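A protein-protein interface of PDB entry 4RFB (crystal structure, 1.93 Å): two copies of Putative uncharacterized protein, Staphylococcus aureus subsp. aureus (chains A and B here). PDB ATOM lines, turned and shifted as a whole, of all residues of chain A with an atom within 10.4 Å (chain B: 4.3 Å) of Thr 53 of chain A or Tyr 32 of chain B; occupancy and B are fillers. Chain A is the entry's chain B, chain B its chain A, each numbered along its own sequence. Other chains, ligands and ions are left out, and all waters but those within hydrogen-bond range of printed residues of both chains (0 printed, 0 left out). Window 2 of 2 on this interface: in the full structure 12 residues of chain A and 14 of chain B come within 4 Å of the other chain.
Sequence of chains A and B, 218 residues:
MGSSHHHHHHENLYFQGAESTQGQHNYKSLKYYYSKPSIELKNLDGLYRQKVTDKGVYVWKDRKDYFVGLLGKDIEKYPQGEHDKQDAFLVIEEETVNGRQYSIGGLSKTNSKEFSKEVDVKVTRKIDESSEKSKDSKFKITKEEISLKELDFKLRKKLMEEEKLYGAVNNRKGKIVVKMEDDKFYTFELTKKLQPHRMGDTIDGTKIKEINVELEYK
OE1 of Glu 94 of chain B sits close to OH of Tyr 32 of chain B. The side-chain amino group of Lys 36 of chain B is in salt-bridge range of the side-chain carboxylate of Glu 94 of chain B, at 2.7 Å. The backbone carbonyl oxygen (O) of Val 52 of chain A sits at hydrogen-bond distance from the guanidinium group (NH2) of Arg 49 of chain A (3.1 Å).
Lys 28 of chain B touches Val 52 of chain A. Ser 29 of chain B touches Val 52 of chain A. Tyr 32 of chain B touches Thr 53 of chain A (CD2 to CG2, 3.6 Å). Thr 53 of chain A touches Glu 94 of chain B.
Printed residues of chain B within 4 Å of Val 52 of chain A: Lys 28 (3.9 Å) and Ser 29 (3.4 Å). Of the printed residues of chain B, Thr 53 of chain A touches Tyr 32 (3.6 Å) and Glu 94 (3.9 Å). Of the printed residues of chain A, Lys 28 of chain B touches Val 52. Ser 29 of chain B touches just one residue of chain A: Val 52. Tyr 32 of chain B touches one residue of chain A. No residue of chain A comes within 4 Å of Ser 35 of chain B. No residue of chain A comes within 4 Å of Lys 36 of chain B. Printed residues of chain A within 4 Å of Glu 94 of chain B: Thr 53. The nearest printed residue of chain B that does not touch Thr 53 of chain A is Ser 29 of chain B (4.4 Å). The nearest printed residue of chain A that does not touch Glu 94 of chain B is Asp 54 of chain A (4.2 Å).
Of the 10 printed residues of chain B, 4 touch a printed residue of chain A. Of the 20 printed residues of chain A, 2 touch a printed residue of chain B. Hydrophobic or aromatic side chains of chain A that line the printed part of chain B: Val 52. Among the printed residues, 4 pairs touch across the chains.
No position is printed for both chains. Of the 4 pairs that touch across the chains among the printed residues, none has its exchanged pair printed and touching as well.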
ATOM      1  N   TYR A  48      -4.318 -19.793  12.304  1.00  0.00           N
ATOM      2  CA  TYR A  48      -3.457 -18.707  12.666  1.00  0.00           C
ATOM      3  C   TYR A  48      -2.612 -18.147  11.505  1.00  0.00           C
ATOM      4  O   TYR A  48      -1.917 -18.894  10.812  1.00  0.00           O
ATOM      5  CB  TYR A  48      -2.563 -19.197  13.774  1.00  0.00           C
ATOM      6  CG  TYR A  48      -1.706 -18.120  14.313  1.00  0.00           C
ATOM      7  CD1 TYR A  48      -2.249 -17.097  15.089  1.00  0.00           C
ATOM      8  CD2 TYR A  48      -0.358 -18.101  14.055  1.00  0.00           C
ATOM      9  CE1 TYR A  48      -1.464 -16.086  15.578  1.00  0.00           C
ATOM     10  CE2 TYR A  48       0.438 -17.097  14.557  1.00  0.00           C
ATOM     11  CZ  TYR A  48      -0.124 -16.093  15.312  1.00  0.00           C
ATOM     12  OH  TYR A  48       0.687 -15.103  15.803  1.00  0.00           O
ATOM     13  N   ARG A  49      -2.729 -16.840  11.289  1.00  0.00           N
ATOM     14  CA  ARG A  49      -1.963 -16.086  10.283  1.00  0.00           C
ATOM     15  C   ARG A  49      -0.839 -15.437  11.103  1.00  0.00           C
ATOM     16  O   ARG A  49      -1.063 -14.413  11.765  1.00  0.00           O
ATOM     17  CB  ARG A  49      -2.850 -15.021   9.651  1.00  0.00           C
ATOM     18  CG  ARG A  49      -2.154 -14.068   8.699  1.00  0.00           C
ATOM     19  CD  ARG A  49      -1.951 -14.635   7.308  1.00  0.00           C
ATOM     20  NE  ARG A  49      -1.385 -13.625   6.403  1.00  0.00           N
ATOM     21  CZ  ARG A  49      -2.067 -12.666   5.786  1.00  0.00           C
ATOM     22  NH1 ARG A  49      -3.366 -12.522   5.961  1.00  0.00           N
ATOM     23  NH2 ARG A  49      -1.432 -11.806   4.997  1.00  0.00           N
ATOM     24  N   GLN A  50       0.362 -15.994  11.057  1.00  0.00           N
ATOM     25  CA  GLN A  50       1.406 -15.562  12.027  1.00  0.00           C
ATOM     26  C   GLN A  50       1.958 -14.170  11.855  1.00  0.00           C
ATOM     27  O   GLN A  50       2.029 -13.382  12.816  1.00  0.00           O
ATOM     28  CB  GLN A  50       2.551 -16.594  12.122  1.00  0.00           C
ATOM     29  CG  GLN A  50       3.562 -16.292  13.238  1.00  0.00           C
ATOM     30  CD  GLN A  50       4.530 -17.437  13.507  1.00  0.00           C
ATOM     31  OE1 GLN A  50       4.844 -18.231  12.619  1.00  0.00           O
ATOM     32  NE2 GLN A  50       5.013 -17.515  14.735  1.00  0.00           N
ATOM     33  N   LYS A  51       2.383 -13.877  10.647  1.00  0.00           N
ATOM     34  CA  LYS A  51       2.922 -12.581  10.322  1.00  0.00           C
ATOM     35  C   LYS A  51       2.068 -12.226   9.151  1.00  0.00           C
ATOM     36  O   LYS A  51       1.413 -13.115   8.593  1.00  0.00           O
ATOM     37  CB  LYS A  51       4.391 -12.706   9.934  1.00  0.00           C
ATOM     38  CG  LYS A  51       5.233 -13.252  11.086  1.00  0.00           C
ATOM     39  CD  LYS A  51       6.456 -14.047  10.644  1.00  0.00           C
ATOM     40  CE  LYS A  51       7.039 -14.806  11.835  1.00  0.00           C
ATOM     41  NZ  LYS A  51       8.007 -15.870  11.455  1.00  0.00           N
ATOM     42  N   VAL A  52       2.058 -10.947   8.793  1.00  0.00           N
ATOM     43  CA  VAL A  52       1.272 -10.462   7.656  1.00  0.00           C
ATOM     44  C   VAL A  52       2.037 -10.821   6.384  1.00  0.00           C
ATOM     45  O   VAL A  52       1.511 -10.725   5.274  1.00  0.00           O
ATOM     46  CB  VAL A  52       1.069  -8.927   7.702  1.00  0.00           C
ATOM     47  CG1 VAL A  52       0.683  -8.482   9.103  1.00  0.00           C
ATOM     48  CG2 VAL A  52       2.333  -8.191   7.275  1.00  0.00           C
ATOM     49  N   THR A  53       3.303 -11.183   6.569  1.00  0.00           N
ATOM     50  CA  THR A  53       4.168 -11.586   5.486  1.00  0.00           C
ATOM     51  C   THR A  53       3.742 -12.975   4.952  1.00  0.00           C
ATOM     52  O   THR A  53       3.574 -13.158   3.750  1.00  0.00           O
ATOM     53  CB  THR A  53       5.644 -11.529   5.942  1.00  0.00           C
ATOM     54  OG1 THR A  53       5.805 -12.229   7.179  1.00  0.00           O
ATOM     55  CG2 THR A  53       6.060 -10.075   6.180  1.00  0.00           C
ATOM     56  N   ASP A  54       3.516 -13.930   5.844  1.00  0.00           N
ATOM     57  CA  ASP A  54       3.100 -15.291   5.440  1.00  0.00           C
ATOM     58  C   ASP A  54       2.072 -15.348   4.259  1.00  0.00           C
ATOM     59  O   ASP A  54       1.255 -14.423   4.092  1.00  0.00           O
ATOM     60  CB  ASP A  54       2.566 -16.039   6.668  1.00  0.00           C
ATOM     61  CG  ASP A  54       3.640 -16.230   7.758  1.00  0.00           C
ATOM     62  OD1 ASP A  54       4.773 -15.722   7.571  1.00  0.00           O
ATOM     63  OD2 ASP A  54       3.351 -16.886   8.794  1.00  0.00           O
ATOM     64  N   LYS A  55       2.169 -16.430   3.455  1.00  0.00           N
ATOM     65  CA  LYS A  55       1.307 -16.747   2.245  1.00  0.00           C
ATOM     66  C   LYS A  55       0.367 -17.963   2.482  1.00  0.00           C
ATOM     67  O   LYS A  55       0.076 -18.799   1.603  1.00  0.00           O
ATOM     68  CB  LYS A  55       2.157 -17.048   1.025  1.00  0.00           C
ATOM     69  CG  LYS A  55       3.281 -18.087   1.188  1.00  0.00           C
ATOM     70  CD  LYS A  55       2.878 -19.562   1.246  1.00  0.00           C
ATOM     71  CE  LYS A  55       4.128 -20.419   1.062  1.00  0.00           C
ATOM     72  NZ  LYS A  55       3.875 -21.886   1.034  1.00  0.00           N
ATOM     73  N   GLY A  56      -0.096 -18.029   3.697  1.00  0.00           N
ATOM     74  CA  GLY A  56      -0.992 -19.054   4.119  1.00  0.00           C
ATOM     75  C   GLY A  56      -1.095 -18.931   5.609  1.00  0.00           C
ATOM     76  O   GLY A  56      -0.564 -18.000   6.210  1.00  0.00           O
ATOM     77  N   VAL A  57      -1.763 -19.909   6.199  1.00  0.00           N
ATOM     78  CA  VAL A  57      -2.039 -19.909   7.598  1.00  0.00           C
ATOM     79  C   VAL A  57      -1.817 -21.285   8.188  1.00  0.00           C
ATOM     80  O   VAL A  57      -1.854 -22.303   7.492  1.00  0.00           O
ATOM     81  CB  VAL A  57      -3.542 -19.534   7.811  1.00  0.00           C
ATOM     82  CG1 VAL A  57      -3.834 -18.132   7.292  1.00  0.00           C
ATOM     83  CG2 VAL A  57      -4.469 -20.525   7.119  1.00  0.00           C
ATOM     84  N   TYR A  58      -1.561 -21.323   9.476  1.00  0.00           N
ATOM     85  CA  TYR A  58      -1.466 -22.595  10.174  1.00  0.00           C
ATOM     86  C   TYR A  58      -2.855 -23.026  10.634  1.00  0.00           C
ATOM     87  O   TYR A  58      -3.604 -22.207  11.113  1.00  0.00           O
ATOM     88  CB  TYR A  58      -0.590 -22.465  11.396  1.00  0.00           C
ATOM     89  CG  TYR A  58       0.849 -22.095  11.106  1.00  0.00           C
ATOM     90  CD1 TYR A  58       1.237 -20.773  10.938  1.00  0.00           C
ATOM     91  CD2 TYR A  58       1.825 -23.074  11.047  1.00  0.00           C
ATOM     92  CE1 TYR A  58       2.563 -20.444  10.682  1.00  0.00           C
ATOM     93  CE2 TYR A  58       3.149 -22.748  10.823  1.00  0.00           C
ATOM     94  CZ  TYR A  58       3.504 -21.444  10.628  1.00  0.00           C
ATOM     95  OH  TYR A  58       4.830 -21.160  10.386  1.00  0.00           O
ATOM     96  N   PHE A  67      -0.217 -26.605   7.347  1.00  0.00           N
ATOM     97  CA  PHE A  67      -0.077 -25.287   6.799  1.00  0.00           C
ATOM     98  C   PHE A  67      -0.920 -25.257   5.525  1.00  0.00           C
ATOM     99  O   PHE A  67      -0.805 -26.141   4.677  1.00  0.00           O
ATOM    100  CB  PHE A  67       1.384 -24.956   6.510  1.00  0.00           C
ATOM    101  CG  PHE A  67       1.603 -23.499   6.183  1.00  0.00           C
ATOM    102  CD1 PHE A  67       1.708 -22.553   7.199  1.00  0.00           C
ATOM    103  CD2 PHE A  67       1.664 -23.077   4.876  1.00  0.00           C
ATOM    104  CE1 PHE A  67       1.913 -21.207   6.901  1.00  0.00           C
ATOM    105  CE2 PHE A  67       1.873 -21.736   4.566  1.00  0.00           C
ATOM    106  CZ  PHE A  67       2.000 -20.799   5.579  1.00  0.00           C
ATOM    107  N   LEU A  70      -2.849 -19.902   0.698  1.00  0.00           N
ATOM    108  CA  LEU A  70      -4.001 -19.154   0.190  1.00  0.00           C
ATOM    109  C   LEU A  70      -3.444 -18.192  -0.816  1.00  0.00           C
ATOM    110  O   LEU A  70      -2.562 -17.411  -0.469  1.00  0.00           O
ATOM    111  CB  LEU A  70      -4.732 -18.458   1.313  1.00  0.00           C
ATOM    112  CG  LEU A  70      -5.492 -19.368   2.300  1.00  0.00           C
ATOM    113  CD1 LEU A  70      -5.876 -18.596   3.541  1.00  0.00           C
ATOM    114  CD2 LEU A  70      -6.708 -19.938   1.625  1.00  0.00           C
ATOM    115  N   GLY A  72      -3.789 -15.253  -4.063  1.00  0.00           N
ATOM    116  CA  GLY A  72      -4.503 -14.046  -4.443  1.00  0.00           C
ATOM    117  C   GLY A  72      -5.224 -13.413  -3.262  1.00  0.00           C
ATOM    118  O   GLY A  72      -4.645 -13.249  -2.184  1.00  0.00           O
ATOM    119  N   ILE A  75      -6.200 -14.892   0.805  1.00  0.00           N
ATOM    120  CA  ILE A  75      -5.434 -14.600   2.000  1.00  0.00           C
ATOM    121  C   ILE A  75      -6.080 -13.457   2.818  1.00  0.00           C
ATOM    122  O   ILE A  75      -5.999 -13.444   4.054  1.00  0.00           O
ATOM    123  CB  ILE A  75      -3.954 -14.312   1.656  1.00  0.00           C
ATOM    124  CG1 ILE A  75      -3.098 -14.289   2.919  1.00  0.00           C
ATOM    125  CG2 ILE A  75      -3.786 -13.023   0.878  1.00  0.00           C
ATOM    126  CD1 ILE A  75      -3.008 -15.614   3.642  1.00  0.00           C
ATOM    127  N   TYR A  78      -8.212 -13.802   6.211  1.00  0.00           N
ATOM    128  CA  TYR A  78      -7.607 -14.110   7.503  1.00  0.00           C
ATOM    129  C   TYR A  78      -6.451 -13.167   7.789  1.00  0.00           C
ATOM    130  O   TYR A  78      -5.300 -13.509   7.535  1.00  0.00           O
ATOM    131  CB  TYR A  78      -7.138 -15.569   7.537  1.00  0.00           C
ATOM    132  CG  TYR A  78      -8.244 -16.572   7.218  1.00  0.00           C
ATOM    133  CD1 TYR A  78      -9.275 -16.801   8.113  1.00  0.00           C
ATOM    134  CD2 TYR A  78      -8.270 -17.254   6.002  1.00  0.00           C
ATOM    135  CE1 TYR A  78     -10.291 -17.698   7.836  1.00  0.00           C
ATOM    136  CE2 TYR A  78      -9.271 -18.158   5.720  1.00  0.00           C
ATOM    137  CZ  TYR A  78     -10.288 -18.365   6.628  1.00  0.00           C
ATOM    138  OH  TYR A  78     -11.307 -19.248   6.355  1.00  0.00           O
ATOM    139  N   PRO A  79      -6.756 -11.974   8.334  1.00  0.00           N
ATOM    140  CA  PRO A  79      -5.679 -11.044   8.692  1.00  0.00           C
ATOM    141  C   PRO A  79      -4.850 -11.575   9.854  1.00  0.00           C
ATOM    142  O   PRO A  79      -5.288 -12.479  10.569  1.00  0.00           O
ATOM    143  CB  PRO A  79      -6.415  -9.751   9.090  1.00  0.00           C
ATOM    144  CG  PRO A  79      -7.831 -10.143   9.297  1.00  0.00           C
ATOM    145  CD  PRO A  79      -8.087 -11.363   8.464  1.00  0.00           C
ATOM    146  N   GLN A  80      -3.683 -10.982  10.053  1.00  0.00           N
ATOM    147  CA  GLN A  80      -2.750 -11.428  11.074  1.00  0.00           C
ATOM    148  C   GLN A  80      -3.487 -11.736  12.379  1.00  0.00           C
ATOM    149  O   GLN A  80      -4.308 -10.951  12.848  1.00  0.00           O
ATOM    150  CB  GLN A  80      -1.663 -10.376  11.270  1.00  0.00           C
ATOM    151  CG  GLN A  80      -0.419 -10.895  11.966  1.00  0.00           C
ATOM    152  CD  GLN A  80      -0.653 -11.188  13.425  1.00  0.00           C
ATOM    153  OE1 GLN A  80      -1.224 -10.366  14.145  1.00  0.00           O
ATOM    154  NE2 GLN A  80      -0.207 -12.356  13.881  1.00  0.00           N
ATOM    155  N   GLY A  81      -3.188 -12.881  12.961  1.00  0.00           N
ATOM    156  CA  GLY A  81      -3.821 -13.286  14.219  1.00  0.00           C
ATOM    157  C   GLY A  81      -4.556 -14.602  14.143  1.00  0.00           C
ATOM    158  O   GLY A  81      -4.504 -15.306  13.136  1.00  0.00           O
ATOM    159  N   ASN A  98       7.275 -25.354   6.311  1.00  0.00           N
ATOM    160  CA  ASN A  98       7.546 -25.139   7.750  1.00  0.00           C
ATOM    161  C   ASN A  98       7.418 -26.387   8.574  1.00  0.00           C
ATOM    162  O   ASN A  98       6.904 -26.361   9.702  1.00  0.00           O
ATOM    163  CB  ASN A  98       6.674 -24.006   8.311  1.00  0.00           C
ATOM    164  CG  ASN A  98       7.106 -22.657   7.791  1.00  0.00           C
ATOM    165  OD1 ASN A  98       8.275 -22.477   7.449  1.00  0.00           O
ATOM    166  ND2 ASN A  98       6.181 -21.708   7.727  1.00  0.00           N
ATOM    167  N   LYS B  28       3.701  -2.508   5.192  1.00  0.00           N
ATOM    168  CA  LYS B  28       4.499  -3.380   6.019  1.00  0.00           C
ATOM    169  C   LYS B  28       5.105  -4.523   5.225  1.00  0.00           C
ATOM    170  O   LYS B  28       6.297  -4.802   5.345  1.00  0.00           O
ATOM    171  CB  LYS B  28       3.650  -3.895   7.188  1.00  0.00           C
ATOM    172  CG  LYS B  28       4.383  -4.825   8.128  1.00  0.00           C
ATOM    173  CD  LYS B  28       3.557  -5.138   9.371  1.00  0.00           C
ATOM    174  CE  LYS B  28       4.208  -6.252  10.177  1.00  0.00           C
ATOM    175  NZ  LYS B  28       5.644  -5.971  10.472  1.00  0.00           N
ATOM    176  N   SER B  29       4.293  -5.190   4.410  1.00  0.00           N
ATOM    177  CA  SER B  29       4.796  -6.319   3.603  1.00  0.00           C
ATOM    178  C   SER B  29       5.764  -5.858   2.517  1.00  0.00           C
ATOM    179  O   SER B  29       6.789  -6.499   2.284  1.00  0.00           O
ATOM    180  CB  SER B  29       3.646  -7.110   2.965  1.00  0.00           C
ATOM    181  OG  SER B  29       2.823  -7.704   3.957  1.00  0.00           O
ATOM    182  N   LEU B  30       5.427  -4.749   1.867  1.00  0.00           N
ATOM    183  CA  LEU B  30       6.258  -4.187   0.793  1.00  0.00           C
ATOM    184  C   LEU B  30       7.642  -3.852   1.302  1.00  0.00           C
ATOM    185  O   LEU B  30       8.637  -4.313   0.772  1.00  0.00           O
ATOM    186  CB  LEU B  30       5.628  -2.903   0.246  1.00  0.00           C
ATOM    187  CG  LEU B  30       4.336  -2.987  -0.559  1.00  0.00           C
ATOM    188  CD1 LEU B  30       3.767  -1.608  -0.764  1.00  0.00           C
ATOM    189  CD2 LEU B  30       4.593  -3.649  -1.899  1.00  0.00           C
ATOM    190  N   LYS B  31       7.699  -3.030   2.335  1.00  0.00           N
ATOM    191  CA  LYS B  31       8.980  -2.625   2.886  1.00  0.00           C
ATOM    192  C   LYS B  31       9.765  -3.862   3.275  1.00  0.00           C
ATOM    193  O   LYS B  31      10.960  -3.934   3.071  1.00  0.00           O
ATOM    194  CB  LYS B  31       8.769  -1.705   4.101  1.00  0.00           C
ATOM    195  CG  LYS B  31      10.044  -1.141   4.730  1.00  0.00           C
ATOM    196  CD  LYS B  31      10.936  -0.464   3.699  1.00  0.00           C
ATOM    197  CE  LYS B  31      12.060   0.359   4.319  1.00  0.00           C
ATOM    198  NZ  LYS B  31      11.554   1.581   5.018  1.00  0.00           N
ATOM    199  N   TYR B  32       9.072  -4.871   3.789  1.00  0.00           N
ATOM    200  CA  TYR B  32       9.735  -6.096   4.250  1.00  0.00           C
ATOM    201  C   TYR B  32      10.345  -6.950   3.134  1.00  0.00           C
ATOM    202  O   TYR B  32      11.521  -7.328   3.219  1.00  0.00           O
ATOM    203  CB  TYR B  32       8.768  -6.912   5.111  1.00  0.00           C
ATOM    204  CG  TYR B  32       9.432  -7.997   5.903  1.00  0.00           C
ATOM    205  CD1 TYR B  32       9.978  -7.735   7.155  1.00  0.00           C
ATOM    206  CD2 TYR B  32       9.516  -9.286   5.406  1.00  0.00           C
ATOM    207  CE1 TYR B  32      10.596  -8.733   7.886  1.00  0.00           C
ATOM    208  CE2 TYR B  32      10.122 -10.290   6.122  1.00  0.00           C
ATOM    209  CZ  TYR B  32      10.664 -10.017   7.358  1.00  0.00           C
ATOM    210  OH  TYR B  32      11.262 -11.022   8.067  1.00  0.00           O
ATOM    211  N   TYR B  33       9.565  -7.297   2.105  1.00  0.00           N
ATOM    212  CA  TYR B  33      10.092  -8.093   1.001  1.00  0.00           C
ATOM    213  C   TYR B  33      11.177  -7.329   0.247  1.00  0.00           C
ATOM    214  O   TYR B  33      12.281  -7.862  -0.012  1.00  0.00           O
ATOM    215  CB  TYR B  33       8.949  -8.545   0.013  1.00  0.00           C
ATOM    216  CG  TYR B  33       9.404  -9.263  -1.277  1.00  0.00           C
ATOM    217  CD1 TYR B  33       9.744 -10.646  -1.302  1.00  0.00           C
ATOM    218  CD2 TYR B  33       9.454  -8.592  -2.474  1.00  0.00           C
ATOM    219  CE1 TYR B  33      10.139 -11.285  -2.502  1.00  0.00           C
ATOM    220  CE2 TYR B  33       9.851  -9.219  -3.666  1.00  0.00           C
ATOM    221  CZ  TYR B  33      10.205 -10.560  -3.692  1.00  0.00           C
ATOM    222  OH  TYR B  33      10.618 -11.140  -4.950  1.00  0.00           O
ATOM    223  N   TYR B  34      10.882  -6.079  -0.116  1.00  0.00           N
ATOM    224  CA  TYR B  34      11.815  -5.339  -0.968  1.00  0.00           C
ATOM    225  C   TYR B  34      13.091  -4.890  -0.274  1.00  0.00           C
ATOM    226  O   TYR B  34      14.010  -4.462  -0.937  1.00  0.00           O
ATOM    227  CB  TYR B  34      11.105  -4.227  -1.754  1.00  0.00           C
ATOM    228  CG  TYR B  34      10.168  -4.839  -2.800  1.00  0.00           C
ATOM    229  CD1 TYR B  34      10.680  -5.422  -3.941  1.00  0.00           C
ATOM    230  CD2 TYR B  34       8.777  -4.862  -2.609  1.00  0.00           C
ATOM    231  CE1 TYR B  34       9.850  -6.014  -4.883  1.00  0.00           C
ATOM    232  CE2 TYR B  34       7.934  -5.447  -3.541  1.00  0.00           C
ATOM    233  CZ  TYR B  34       8.468  -6.047  -4.667  1.00  0.00           C
ATOM    234  OH  TYR B  34       7.643  -6.628  -5.607  1.00  0.00           O
ATOM    235  N   SER B  35      13.141  -5.031   1.050  1.00  0.00           N
ATOM    236  CA  SER B  35      14.340  -4.718   1.810  1.00  0.00           C
ATOM    237  C   SER B  35      15.239  -5.937   1.941  1.00  0.00           C
ATOM    238  O   SER B  35      16.337  -5.836   2.466  1.00  0.00           O
ATOM    239  CB  SER B  35      13.979  -4.178   3.213  1.00  0.00           C
ATOM    240  OG  SER B  35      13.251  -2.959   3.089  1.00  0.00           O
ATOM    241  N   LYS B  36      14.780  -7.102   1.493  1.00  0.00           N
ATOM    242  CA  LYS B  36      15.612  -8.308   1.582  1.00  0.00           C
ATOM    243  C   LYS B  36      16.738  -8.271   0.589  1.00  0.00           C
ATOM    244  O   LYS B  36      16.617  -7.605  -0.434  1.00  0.00           O
ATOM    245  CB  LYS B  36      14.777  -9.543   1.306  1.00  0.00           C
ATOM    246  CG  LYS B  36      13.735  -9.819   2.368  1.00  0.00           C
ATOM    247  CD  LYS B  36      12.982 -11.116   2.078  1.00  0.00           C
ATOM    248  CE  LYS B  36      12.234 -11.584   3.319  1.00  0.00           C
ATOM    249  NZ  LYS B  36      11.639 -12.918   3.145  1.00  0.00           N
ATOM    250  N   GLU B  94       9.895 -16.330   3.806  1.00  0.00           N
ATOM    251  CA  GLU B  94       9.791 -16.625   5.224  1.00  0.00           C
ATOM    252  C   GLU B  94       9.630 -18.107   5.511  1.00  0.00           C
ATOM    253  O   GLU B  94      10.157 -18.602   6.489  1.00  0.00           O
ATOM    254  CB  GLU B  94       8.608 -15.856   5.827  1.00  0.00           C
ATOM    255  CG  GLU B  94       8.806 -14.344   5.762  1.00  0.00           C
ATOM    256  CD  GLU B  94      10.113 -13.953   6.400  1.00  0.00           C
ATOM    257  OE1 GLU B  94      10.962 -13.342   5.713  1.00  0.00           O
ATOM    258  OE2 GLU B  94      10.312 -14.325   7.576  1.00  0.00           O
